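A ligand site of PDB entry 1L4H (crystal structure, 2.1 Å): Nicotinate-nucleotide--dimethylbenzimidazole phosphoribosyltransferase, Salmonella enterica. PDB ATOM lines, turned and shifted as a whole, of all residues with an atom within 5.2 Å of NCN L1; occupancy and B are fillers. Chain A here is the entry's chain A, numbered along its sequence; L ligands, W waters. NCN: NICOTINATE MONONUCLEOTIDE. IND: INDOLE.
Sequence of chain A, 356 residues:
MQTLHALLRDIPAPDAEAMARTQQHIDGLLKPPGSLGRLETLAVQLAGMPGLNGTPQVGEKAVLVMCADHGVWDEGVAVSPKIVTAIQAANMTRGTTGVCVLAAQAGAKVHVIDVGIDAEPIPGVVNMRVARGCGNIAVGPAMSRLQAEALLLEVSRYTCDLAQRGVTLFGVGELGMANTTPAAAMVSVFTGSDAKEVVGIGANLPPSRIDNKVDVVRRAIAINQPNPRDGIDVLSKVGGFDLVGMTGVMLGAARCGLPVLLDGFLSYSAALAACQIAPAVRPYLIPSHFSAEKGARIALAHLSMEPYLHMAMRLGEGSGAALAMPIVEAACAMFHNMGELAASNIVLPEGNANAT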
ATOM      1  N   VAL A  77     -27.835 -15.915 -18.231  1.00  0.00           N
ATOM      2  CA  VAL A  77     -27.014 -14.721 -18.440  1.00  0.00           C
ATOM      3  C   VAL A  77     -25.608 -15.018 -18.993  1.00  0.00           C
ATOM      4  O   VAL A  77     -24.829 -14.092 -19.212  1.00  0.00           O
ATOM      5  CB  VAL A  77     -26.865 -13.878 -17.122  1.00  0.00           C
ATOM      6  CG1 VAL A  77     -28.229 -13.403 -16.642  1.00  0.00           C
ATOM      7  CG2 VAL A  77     -26.184 -14.723 -16.043  1.00  0.00           C
ATOM      8  N   ALA A  78     -25.288 -16.300 -19.193  1.00  0.00           N
ATOM      9  CA  ALA A  78     -23.967 -16.697 -19.710  1.00  0.00           C
ATOM     10  C   ALA A  78     -24.062 -17.855 -20.708  1.00  0.00           C
ATOM     11  O   ALA A  78     -24.770 -18.831 -20.460  1.00  0.00           O
ATOM     12  CB  ALA A  78     -23.046 -17.105 -18.561  1.00  0.00           C
ATOM     13  N   SER A  80     -21.372 -19.656 -21.716  1.00  0.00           N
ATOM     14  CA  SER A  80     -20.356 -20.680 -21.414  1.00  0.00           C
ATOM     15  C   SER A  80     -20.970 -21.735 -20.495  1.00  0.00           C
ATOM     16  O   SER A  80     -21.684 -21.395 -19.561  1.00  0.00           O
ATOM     17  CB  SER A  80     -19.145 -20.073 -20.688  1.00  0.00           C
ATOM     18  OG  SER A  80     -18.441 -19.131 -21.455  1.00  0.00           O
ATOM     19  N   GLU A 174      -9.916 -13.742 -11.321  1.00  0.00           N
ATOM     20  CA  GLU A 174     -11.034 -14.630 -11.037  1.00  0.00           C
ATOM     21  C   GLU A 174     -11.350 -15.577 -12.182  1.00  0.00           C
ATOM     22  O   GLU A 174     -10.793 -15.495 -13.273  1.00  0.00           O
ATOM     23  CB  GLU A 174     -12.282 -13.810 -10.716  1.00  0.00           C
ATOM     24  CG  GLU A 174     -12.500 -12.596 -11.615  1.00  0.00           C
ATOM     25  CD  GLU A 174     -12.522 -12.944 -13.096  1.00  0.00           C
ATOM     26  OE1 GLU A 174     -13.414 -13.698 -13.531  1.00  0.00           O
ATOM     27  OE2 GLU A 174     -11.640 -12.488 -13.838  1.00  0.00           O
ATOM     28  N   LEU A 175     -12.272 -16.489 -11.899  1.00  0.00           N
ATOM     29  CA  LEU A 175     -12.730 -17.470 -12.842  1.00  0.00           C
ATOM     30  C   LEU A 175     -14.100 -17.890 -12.328  1.00  0.00           C
ATOM     31  O   LEU A 175     -14.219 -18.339 -11.187  1.00  0.00           O
ATOM     32  CB  LEU A 175     -11.772 -18.651 -12.872  1.00  0.00           C
ATOM     33  CG  LEU A 175     -12.113 -19.798 -13.826  1.00  0.00           C
ATOM     34  CD1 LEU A 175     -12.049 -19.273 -15.262  1.00  0.00           C
ATOM     35  CD2 LEU A 175     -11.124 -20.965 -13.636  1.00  0.00           C
ATOM     36  N   GLY A 176     -15.128 -17.712 -13.145  1.00  0.00           N
ATOM     37  CA  GLY A 176     -16.474 -18.094 -12.744  1.00  0.00           C
ATOM     38  C   GLY A 176     -17.496 -17.671 -13.780  1.00  0.00           C
ATOM     39  O   GLY A 176     -17.751 -16.489 -13.976  1.00  0.00           O
ATOM     40  N   MET A 177     -18.080 -18.663 -14.459  1.00  0.00           N
ATOM     41  CA  MET A 177     -19.093 -18.395 -15.477  1.00  0.00           C
ATOM     42  C   MET A 177     -20.234 -17.577 -14.869  1.00  0.00           C
ATOM     43  O   MET A 177     -20.691 -17.851 -13.770  1.00  0.00           O
ATOM     44  CB  MET A 177     -19.628 -19.713 -16.039  1.00  0.00           C
ATOM     45  CG  MET A 177     -18.553 -20.636 -16.597  1.00  0.00           C
ATOM     46  SD  MET A 177     -17.431 -19.809 -17.754  1.00  0.00           S
ATOM     47  CE  MET A 177     -15.870 -19.804 -16.815  1.00  0.00           C
ATOM     48  N   ALA A 178     -20.674 -16.549 -15.605  1.00  0.00           N
ATOM     49  CA  ALA A 178     -21.765 -15.644 -15.192  1.00  0.00           C
ATOM     50  C   ALA A 178     -21.355 -14.546 -14.200  1.00  0.00           C
ATOM     51  O   ALA A 178     -22.203 -13.746 -13.770  1.00  0.00           O
ATOM     52  CB  ALA A 178     -22.942 -16.447 -14.581  1.00  0.00           C
ATOM     53  N   ASN A 179     -20.079 -14.477 -13.833  1.00  0.00           N
ATOM     54  CA  ASN A 179     -19.710 -13.461 -12.850  1.00  0.00           C
ATOM     55  C   ASN A 179     -19.737 -11.987 -13.280  1.00  0.00           C
ATOM     56  O   ASN A 179     -19.578 -11.114 -12.433  1.00  0.00           O
ATOM     57  CB  ASN A 179     -18.380 -13.816 -12.111  1.00  0.00           C
ATOM     58  CG  ASN A 179     -17.147 -13.747 -12.991  1.00  0.00           C
ATOM     59  OD1 ASN A 179     -17.185 -13.270 -14.114  1.00  0.00           O
ATOM     60  ND2 ASN A 179     -16.018 -14.222 -12.441  1.00  0.00           N
ATOM     61  N   THR A 180     -19.972 -11.689 -14.554  1.00  0.00           N
ATOM     62  CA  THR A 180     -20.061 -10.284 -14.927  1.00  0.00           C
ATOM     63  C   THR A 180     -21.459  -9.759 -14.561  1.00  0.00           C
ATOM     64  O   THR A 180     -21.698  -8.548 -14.573  1.00  0.00           O
ATOM     65  CB  THR A 180     -19.775 -10.011 -16.437  1.00  0.00           C
ATOM     66  OG1 THR A 180     -20.740 -10.680 -17.263  1.00  0.00           O
ATOM     67  CG2 THR A 180     -18.373 -10.486 -16.807  1.00  0.00           C
ATOM     68  N   THR A 181     -22.380 -10.661 -14.249  1.00  0.00           N
ATOM     69  CA  THR A 181     -23.718 -10.229 -13.852  1.00  0.00           C
ATOM     70  C   THR A 181     -23.639  -9.648 -12.426  1.00  0.00           C
ATOM     71  O   THR A 181     -23.964  -8.481 -12.224  1.00  0.00           O
ATOM     72  CB  THR A 181     -24.737 -11.394 -13.959  1.00  0.00           C
ATOM     73  OG1 THR A 181     -24.993 -11.651 -15.341  1.00  0.00           O
ATOM     74  CG2 THR A 181     -26.064 -11.054 -13.264  1.00  0.00           C
ATOM     75  N   ILE A 201     -21.392  -7.584 -22.519  1.00  0.00           N
ATOM     76  CA  ILE A 201     -21.591  -8.913 -23.099  1.00  0.00           C
ATOM     77  C   ILE A 201     -20.796 -10.019 -22.420  1.00  0.00           C
ATOM     78  O   ILE A 201     -20.890 -11.185 -22.814  1.00  0.00           O
ATOM     79  CB  ILE A 201     -21.255  -8.936 -24.599  1.00  0.00           C
ATOM     80  CG1 ILE A 201     -19.752  -8.741 -24.787  1.00  0.00           C
ATOM     81  CG2 ILE A 201     -22.054  -7.864 -25.325  1.00  0.00           C
ATOM     82  CD1 ILE A 201     -19.271  -9.027 -26.169  1.00  0.00           C
ATOM     83  N   GLY A 202     -20.005  -9.660 -21.409  1.00  0.00           N
ATOM     84  CA  GLY A 202     -19.204 -10.665 -20.721  1.00  0.00           C
ATOM     85  C   GLY A 202     -18.428 -11.546 -21.677  1.00  0.00           C
ATOM     86  O   GLY A 202     -17.714 -11.044 -22.548  1.00  0.00           O
ATOM     87  N   ALA A 203     -18.544 -12.854 -21.527  1.00  0.00           N
ATOM     88  CA  ALA A 203     -17.839 -13.785 -22.388  1.00  0.00           C
ATOM     89  C   ALA A 203     -18.702 -14.097 -23.623  1.00  0.00           C
ATOM     90  O   ALA A 203     -19.335 -15.145 -23.721  1.00  0.00           O
ATOM     91  CB  ALA A 203     -17.512 -15.073 -21.625  1.00  0.00           C
ATOM     92  N   LYS A 213     -30.260 -10.023 -19.364  1.00  0.00           N
ATOM     93  CA  LYS A 213     -29.206  -9.795 -18.392  1.00  0.00           C
ATOM     94  C   LYS A 213     -29.474  -8.511 -17.598  1.00  0.00           C
ATOM     95  O   LYS A 213     -29.308  -8.484 -16.373  1.00  0.00           O
ATOM     96  CB  LYS A 213     -27.853  -9.734 -19.095  1.00  0.00           C
ATOM     97  CG  LYS A 213     -26.655  -9.695 -18.157  1.00  0.00           C
ATOM     98  CD  LYS A 213     -25.360  -9.937 -18.920  1.00  0.00           C
ATOM     99  CE  LYS A 213     -24.141  -9.688 -18.032  1.00  0.00           C
ATOM    100  NZ  LYS A 213     -22.859  -9.760 -18.795  1.00  0.00           N
ATOM    101  N   ASP A 263      -7.154  -6.147 -12.284  1.00  0.00           N
ATOM    102  CA  ASP A 263      -7.213  -6.804 -13.585  1.00  0.00           C
ATOM    103  C   ASP A 263      -8.274  -6.070 -14.386  1.00  0.00           C
ATOM    104  O   ASP A 263      -8.120  -4.892 -14.689  1.00  0.00           O
ATOM    105  CB  ASP A 263      -7.558  -8.312 -13.437  1.00  0.00           C
ATOM    106  CG  ASP A 263      -7.558  -9.057 -14.789  1.00  0.00           C
ATOM    107  OD1 ASP A 263      -6.756  -8.709 -15.678  1.00  0.00           O
ATOM    108  OD2 ASP A 263      -8.338 -10.028 -14.944  1.00  0.00           O
ATOM    109  N   GLY A 264      -9.363  -6.765 -14.711  1.00  0.00           N
ATOM    110  CA  GLY A 264     -10.430  -6.148 -15.470  1.00  0.00           C
ATOM    111  C   GLY A 264     -11.702  -5.792 -14.725  1.00  0.00           C
ATOM    112  O   GLY A 264     -11.683  -5.492 -13.525  1.00  0.00           O
ATOM    113  N   PHE A 265     -12.814  -5.852 -15.450  1.00  0.00           N
ATOM    114  CA  PHE A 265     -14.126  -5.489 -14.928  1.00  0.00           C
ATOM    115  C   PHE A 265     -14.525  -6.079 -13.568  1.00  0.00           C
ATOM    116  O   PHE A 265     -15.051  -5.381 -12.719  1.00  0.00           O
ATOM    117  CB  PHE A 265     -15.218  -5.826 -15.957  1.00  0.00           C
ATOM    118  CG  PHE A 265     -16.561  -5.256 -15.596  1.00  0.00           C
ATOM    119  CD1 PHE A 265     -17.644  -6.094 -15.332  1.00  0.00           C
ATOM    120  CD2 PHE A 265     -16.745  -3.873 -15.514  1.00  0.00           C
ATOM    121  CE1 PHE A 265     -18.890  -5.556 -14.980  1.00  0.00           C
ATOM    122  CE2 PHE A 265     -17.991  -3.334 -15.162  1.00  0.00           C
ATOM    123  CZ  PHE A 265     -19.059  -4.172 -14.895  1.00  0.00           C
ATOM    124  N   LEU A 266     -14.293  -7.385 -13.394  1.00  0.00           N
ATOM    125  CA  LEU A 266     -14.652  -8.042 -12.143  1.00  0.00           C
ATOM    126  C   LEU A 266     -13.836  -7.435 -10.980  1.00  0.00           C
ATOM    127  O   LEU A 266     -14.366  -7.182  -9.910  1.00  0.00           O
ATOM    128  CB  LEU A 266     -14.384  -9.550 -12.237  1.00  0.00           C
ATOM    129  CG  LEU A 266     -15.198 -10.461 -13.193  1.00  0.00           C
ATOM    130  CD1 LEU A 266     -16.681 -10.168 -13.053  1.00  0.00           C
ATOM    131  CD2 LEU A 266     -14.784 -10.250 -14.631  1.00  0.00           C
ATOM    132  N   HIS A 289      -5.024  -2.680 -16.943  1.00  0.00           N
ATOM    133  CA  HIS A 289      -5.577  -2.355 -18.259  1.00  0.00           C
ATOM    134  C   HIS A 289      -7.006  -1.827 -18.206  1.00  0.00           C
ATOM    135  O   HIS A 289      -7.630  -1.810 -17.149  1.00  0.00           O
ATOM    136  CB  HIS A 289      -5.539  -3.595 -19.162  1.00  0.00           C
ATOM    137  CG  HIS A 289      -6.572  -4.624 -18.846  1.00  0.00           C
ATOM    138  ND1 HIS A 289      -6.564  -5.355 -17.681  1.00  0.00           N
ATOM    139  CD2 HIS A 289      -7.614  -5.100 -19.575  1.00  0.00           C
ATOM    140  CE1 HIS A 289      -7.557  -6.230 -17.703  1.00  0.00           C
ATOM    141  NE2 HIS A 289      -8.206  -6.097 -18.842  1.00  0.00           N
ATOM    142  N   SER A 291     -10.527  -2.627 -19.347  1.00  0.00           N
ATOM    143  CA  SER A 291     -11.414  -3.700 -19.828  1.00  0.00           C
ATOM    144  C   SER A 291     -12.385  -3.252 -20.919  1.00  0.00           C
ATOM    145  O   SER A 291     -12.914  -2.138 -20.883  1.00  0.00           O
ATOM    146  CB  SER A 291     -12.200  -4.276 -18.645  1.00  0.00           C
ATOM    147  OG  SER A 291     -13.193  -5.207 -19.080  1.00  0.00           O
ATOM    148  N   GLU A 293     -15.252  -4.383 -21.266  1.00  0.00           N
ATOM    149  CA  GLU A 293     -16.611  -4.547 -20.768  1.00  0.00           C
ATOM    150  C   GLU A 293     -17.275  -3.167 -20.776  1.00  0.00           C
ATOM    151  O   GLU A 293     -16.643  -2.158 -20.458  1.00  0.00           O
ATOM    152  CB  GLU A 293     -16.581  -5.139 -19.348  1.00  0.00           C
ATOM    153  CG  GLU A 293     -17.918  -5.539 -18.748  1.00  0.00           C
ATOM    154  CD  GLU A 293     -18.527  -6.804 -19.361  1.00  0.00           C
ATOM    155  OE1 GLU A 293     -19.589  -7.209 -18.883  1.00  0.00           O
ATOM    156  OE2 GLU A 293     -17.972  -7.403 -20.297  1.00  0.00           O
ATOM    157  N   MET A 313      -8.918  -6.002 -23.817  1.00  0.00           N
ATOM    158  CA  MET A 313      -8.990  -7.345 -23.256  1.00  0.00           C
ATOM    159  C   MET A 313     -10.234  -7.550 -22.383  1.00  0.00           C
ATOM    160  O   MET A 313     -10.756  -6.604 -21.786  1.00  0.00           O
ATOM    161  CB  MET A 313      -7.725  -7.647 -22.463  1.00  0.00           C
ATOM    162  CG  MET A 313      -6.535  -7.992 -23.317  1.00  0.00           C
ATOM    163  SD  MET A 313      -4.973  -7.801 -22.429  1.00  0.00           S
ATOM    164  CE  MET A 313      -5.037  -9.169 -21.301  1.00  0.00           C
ATOM    165  N   ARG A 314     -10.704  -8.786 -22.339  1.00  0.00           N
ATOM    166  CA  ARG A 314     -11.892  -9.126 -21.554  1.00  0.00           C
ATOM    167  C   ARG A 314     -11.899 -10.630 -21.240  1.00  0.00           C
ATOM    168  O   ARG A 314     -12.926 -11.287 -21.332  1.00  0.00           O
ATOM    169  CB  ARG A 314     -13.161  -8.730 -22.327  1.00  0.00           C
ATOM    170  CG  ARG A 314     -13.180  -9.229 -23.761  1.00  0.00           C
ATOM    171  CD  ARG A 314     -14.387  -8.715 -24.535  1.00  0.00           C
ATOM    172  NE  ARG A 314     -14.368  -9.090 -25.955  1.00  0.00           N
ATOM    173  CZ  ARG A 314     -14.644 -10.292 -26.450  1.00  0.00           C
ATOM    174  NH1 ARG A 314     -14.967 -11.299 -25.645  1.00  0.00           N
ATOM    175  NH2 ARG A 314     -14.601 -10.495 -27.761  1.00  0.00           N
ATOM    176  N   LEU A 315     -10.737 -11.162 -20.892  1.00  0.00           N
ATOM    177  CA  LEU A 315     -10.616 -12.579 -20.573  1.00  0.00           C
ATOM    178  C   LEU A 315     -10.764 -12.824 -19.081  1.00  0.00           C
ATOM    179  O   LEU A 315     -11.418 -13.776 -18.662  1.00  0.00           O
ATOM    180  CB  LEU A 315      -9.258 -13.117 -21.027  1.00  0.00           C
ATOM    181  CG  LEU A 315      -8.825 -14.508 -20.529  1.00  0.00           C
ATOM    182  CD1 LEU A 315      -9.790 -15.606 -21.002  1.00  0.00           C
ATOM    183  CD2 LEU A 315      -7.438 -14.790 -21.066  1.00  0.00           C
ATOM    184  N   GLY A 316     -10.149 -11.971 -18.269  1.00  0.00           N
ATOM    185  CA  GLY A 316     -10.205 -12.147 -16.838  1.00  0.00           C
ATOM    186  C   GLY A 316      -9.007 -12.990 -16.429  1.00  0.00           C
ATOM    187  O   GLY A 316      -7.967 -12.965 -17.095  1.00  0.00           O
ATOM    188  N   GLU A 317      -9.156 -13.754 -15.341  1.00  0.00           N
ATOM    189  CA  GLU A 317      -8.115 -14.628 -14.806  1.00  0.00           C
ATOM    190  C   GLU A 317      -6.933 -13.911 -14.169  1.00  0.00           C
ATOM    191  O   GLU A 317      -6.056 -14.554 -13.586  1.00  0.00           O
ATOM    192  CB  GLU A 317      -7.543 -15.537 -15.899  1.00  0.00           C
ATOM    193  CG  GLU A 317      -8.576 -16.239 -16.735  1.00  0.00           C
ATOM    194  CD  GLU A 317      -7.942 -17.222 -17.696  1.00  0.00           C
ATOM    195  OE1 GLU A 317      -6.702 -17.214 -17.822  1.00  0.00           O
ATOM    196  OE2 GLU A 317      -8.703 -17.985 -18.331  1.00  0.00           O
HETATM  197  P   NCN L   1     -19.756 -14.235 -18.260  1.00  0.00           P
HETATM  198  O1P NCN L   1     -20.465 -13.431 -17.201  1.00  0.00           O
HETATM  199  O2P NCN L   1     -20.401 -14.017 -19.582  1.00  0.00           O
HETATM  200  O3P NCN L   1     -19.827 -15.821 -17.878  1.00  0.00           O
HETATM  201  O5' NCN L   1     -18.237 -13.797 -18.328  1.00  0.00           O
HETATM  202  C5' NCN L   1     -17.443 -13.899 -17.124  1.00  0.00           C
HETATM  203  C4' NCN L   1     -16.271 -14.803 -17.388  1.00  0.00           C
HETATM  204  O4' NCN L   1     -15.499 -14.284 -18.506  1.00  0.00           O
HETATM  205  C3' NCN L   1     -15.322 -14.958 -16.221  1.00  0.00           C
HETATM  206  O3' NCN L   1     -14.822 -16.311 -16.032  1.00  0.00           O
HETATM  207  C2' NCN L   1     -14.226 -13.904 -16.537  1.00  0.00           C
HETATM  208  O2' NCN L   1     -12.936 -14.504 -16.229  1.00  0.00           O
HETATM  209  C1' NCN L   1     -14.404 -13.550 -18.031  1.00  0.00           C
HETATM  210  N1  NCN L   1     -14.583 -12.068 -18.378  1.00  0.00           N
HETATM  211  C6  NCN L   1     -15.619 -11.628 -19.265  1.00  0.00           C
HETATM  212  C5  NCN L   1     -15.638 -10.238 -19.501  1.00  0.00           C
HETATM  213  C4  NCN L   1     -14.747  -9.279 -18.955  1.00  0.00           C
HETATM  214  C3  NCN L   1     -13.735  -9.869 -18.066  1.00  0.00           C
HETATM  215  C2  NCN L   1     -13.660 -11.230 -17.793  1.00  0.00           C
HETATM  216  C7  NCN L   1     -12.858  -8.723 -17.564  1.00  0.00           C
HETATM  217  O7  NCN L   1     -12.944  -7.539 -17.820  1.00  0.00           O
HETATM  218  O8  NCN L   1     -11.939  -9.243 -16.751  1.00  0.00           O
HETATM  219  N1  IND L   2     -11.487 -18.573 -19.498  1.00  0.00           N
HETATM  220  C2  IND L   2     -12.086 -17.608 -18.764  1.00  0.00           C
HETATM  221  C3  IND L   2     -13.424 -17.500 -18.987  1.00  0.00           C
HETATM  222  C4  IND L   2     -14.936 -18.857 -20.589  1.00  0.00           C
HETATM  223  C5  IND L   2     -14.967 -19.901 -21.557  1.00  0.00           C
HETATM  224  C6  IND L   2     -13.770 -20.608 -21.920  1.00  0.00           C
HETATM  225  C7  IND L   2     -12.474 -20.216 -21.247  1.00  0.00           C
HETATM  226  C8  IND L   2     -12.487 -19.161 -20.289  1.00  0.00           C
HETATM  227  C9  IND L   2     -13.703 -18.488 -19.956  1.00  0.00           C
HETATM  228  O   HOH W   1     -22.677 -12.621 -20.090  1.00  0.00           O
HETATM  229  O   HOH W   2     -23.208 -13.131 -16.912  1.00  0.00           O
HETATM  230  O   HOH W   3     -21.347 -15.473 -21.763  1.00  0.00           O
HETATM  231  O   HOH W   4     -11.423  -8.701 -14.011  1.00  0.00           O
HETATM  232  O   HOH W   5      -9.232  -8.961 -17.223  1.00  0.00           O
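The backbone NH (N) of Ala 178 sits at hydrogen-bond distance from an oxygen (O3P) of NCN L1. The side-chain hydroxyl of Ser 291 is in hydrogen-bond range of an oxygen (O7) of NCN L1, 2.7 Å away. The backbone NH (N) of Thr 180 lies within hydrogen-bond range of an oxygen (O1P) of NCN L1, 3.2 Å away. OG1 of Thr 180 sits at hydrogen-bond distance from O1P of NCN L1. An oxygen (O2') of NCN L1 sits at hydrogen-bond distance from the side-chain carboxylate (OE1) of Glu 174 (2.9 Å). N of Phe 265 sits at hydrogen-bond distance from O7 of NCN L1 (2.9 Å). O2P of NCN L1 lies within hydrogen-bond range of N of Ala 203, at 2.9 Å. The backbone carbonyl oxygen (O) of Leu 315 sits at hydrogen-bond distance from an oxygen (O2') of NCN L1, 3.0 Å away. N of Gly 176 lies within hydrogen-bond range of O3' of NCN L1 (3.2 Å). OE2 of Glu 317 lies within hydrogen-bond range of N1 of IND L2.
The side-chain hydroxyl (OG) of Ser 291 sits close to the backbone NH (N) of Glu 293, 3.1 Å away. The side-chain hydroxyl (OG1) of Thr 180 is in hydrogen-bond range of the side-chain amino group (NZ) of Lys 213 (2.8 Å). The side-chain carboxylate (OE1) of Glu 174 lies within hydrogen-bond range of the side-chain amide nitrogen (ND2) of Asn 179 (2.9 Å). N of Glu 317 lies within hydrogen-bond range of O of Glu 174 (3.2 Å). The backbone carbonyl oxygen of Gly 176 lies close to the side-chain amide nitrogen of Asn 179, at 3.2 Å. The backbone NH of Gly 202 is in hydrogen-bond range of the side-chain carboxylate of Glu 293, 3.2 Å away.
The backbone carbonyl oxygen of Arg 314 lies close to a nitrogen (N1) of NCN L1. CB of Ala 78 touches O3P of NCN L1 (3.5 Å). Leu 175 touches NCN L1. Met 177 touches NCN L1. OD1 of Asn 179 touches C5' of NCN L1, at 3.1 Å. Gly 202 touches NCN L1. CA of Gly 264 touches O8 of NCN L1, 3.7 Å away. CD2 of Leu 266 touches C2 of NCN L1 (3.5 Å). Glu 293 touches NCN L1. Gly 316 touches NCN L1. Glu 317 touches NCN L1. Hydrophobic or aromatic side chains that line NCN L1: Ala 78, Met 177, Ala 203, Phe 265 and Leu 266. Within 4 Å of NCN L1: Ala 78, Glu 174, Leu 175, Gly 176, Met 177, Ala 178, Asn 179, Thr 180, Gly 202, Ala 203, Gly 264, Phe 265, Leu 266, Ser 291, Glu 293, Arg 314, Leu 315, Gly 316 and Glu 317. The nearest printed residue that does not touch NCN L1 is Asp 263 (4.1 Å).
Water W1 lies within hydrogen-bond range of O2P of NCN L1, O of Val 77 and NZ of Lys 213. Water W5 lies within hydrogen-bond range of the side-chain carboxylate of Asp 263 (2.7 Å), an oxygen (O8) of NCN L1 (2.8 Å), the backbone NH of Gly 316 (3.3 Å), the backbone NH of Gly 264 (3.3 Å) and a ring nitrogen (NE2) of His 289 (3.4 Å). Water W2 lies within hydrogen-bond range of O1P of NCN L1 (2.8 Å), OG1 of Thr 181 (2.8 Å), O of Val 77 (3.0 Å), O of Ala 178 (3.4 Å) and OG1 of Thr 180 (3.5 Å). Water W3 bridges O2P of NCN L1 and O of Ala 203.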
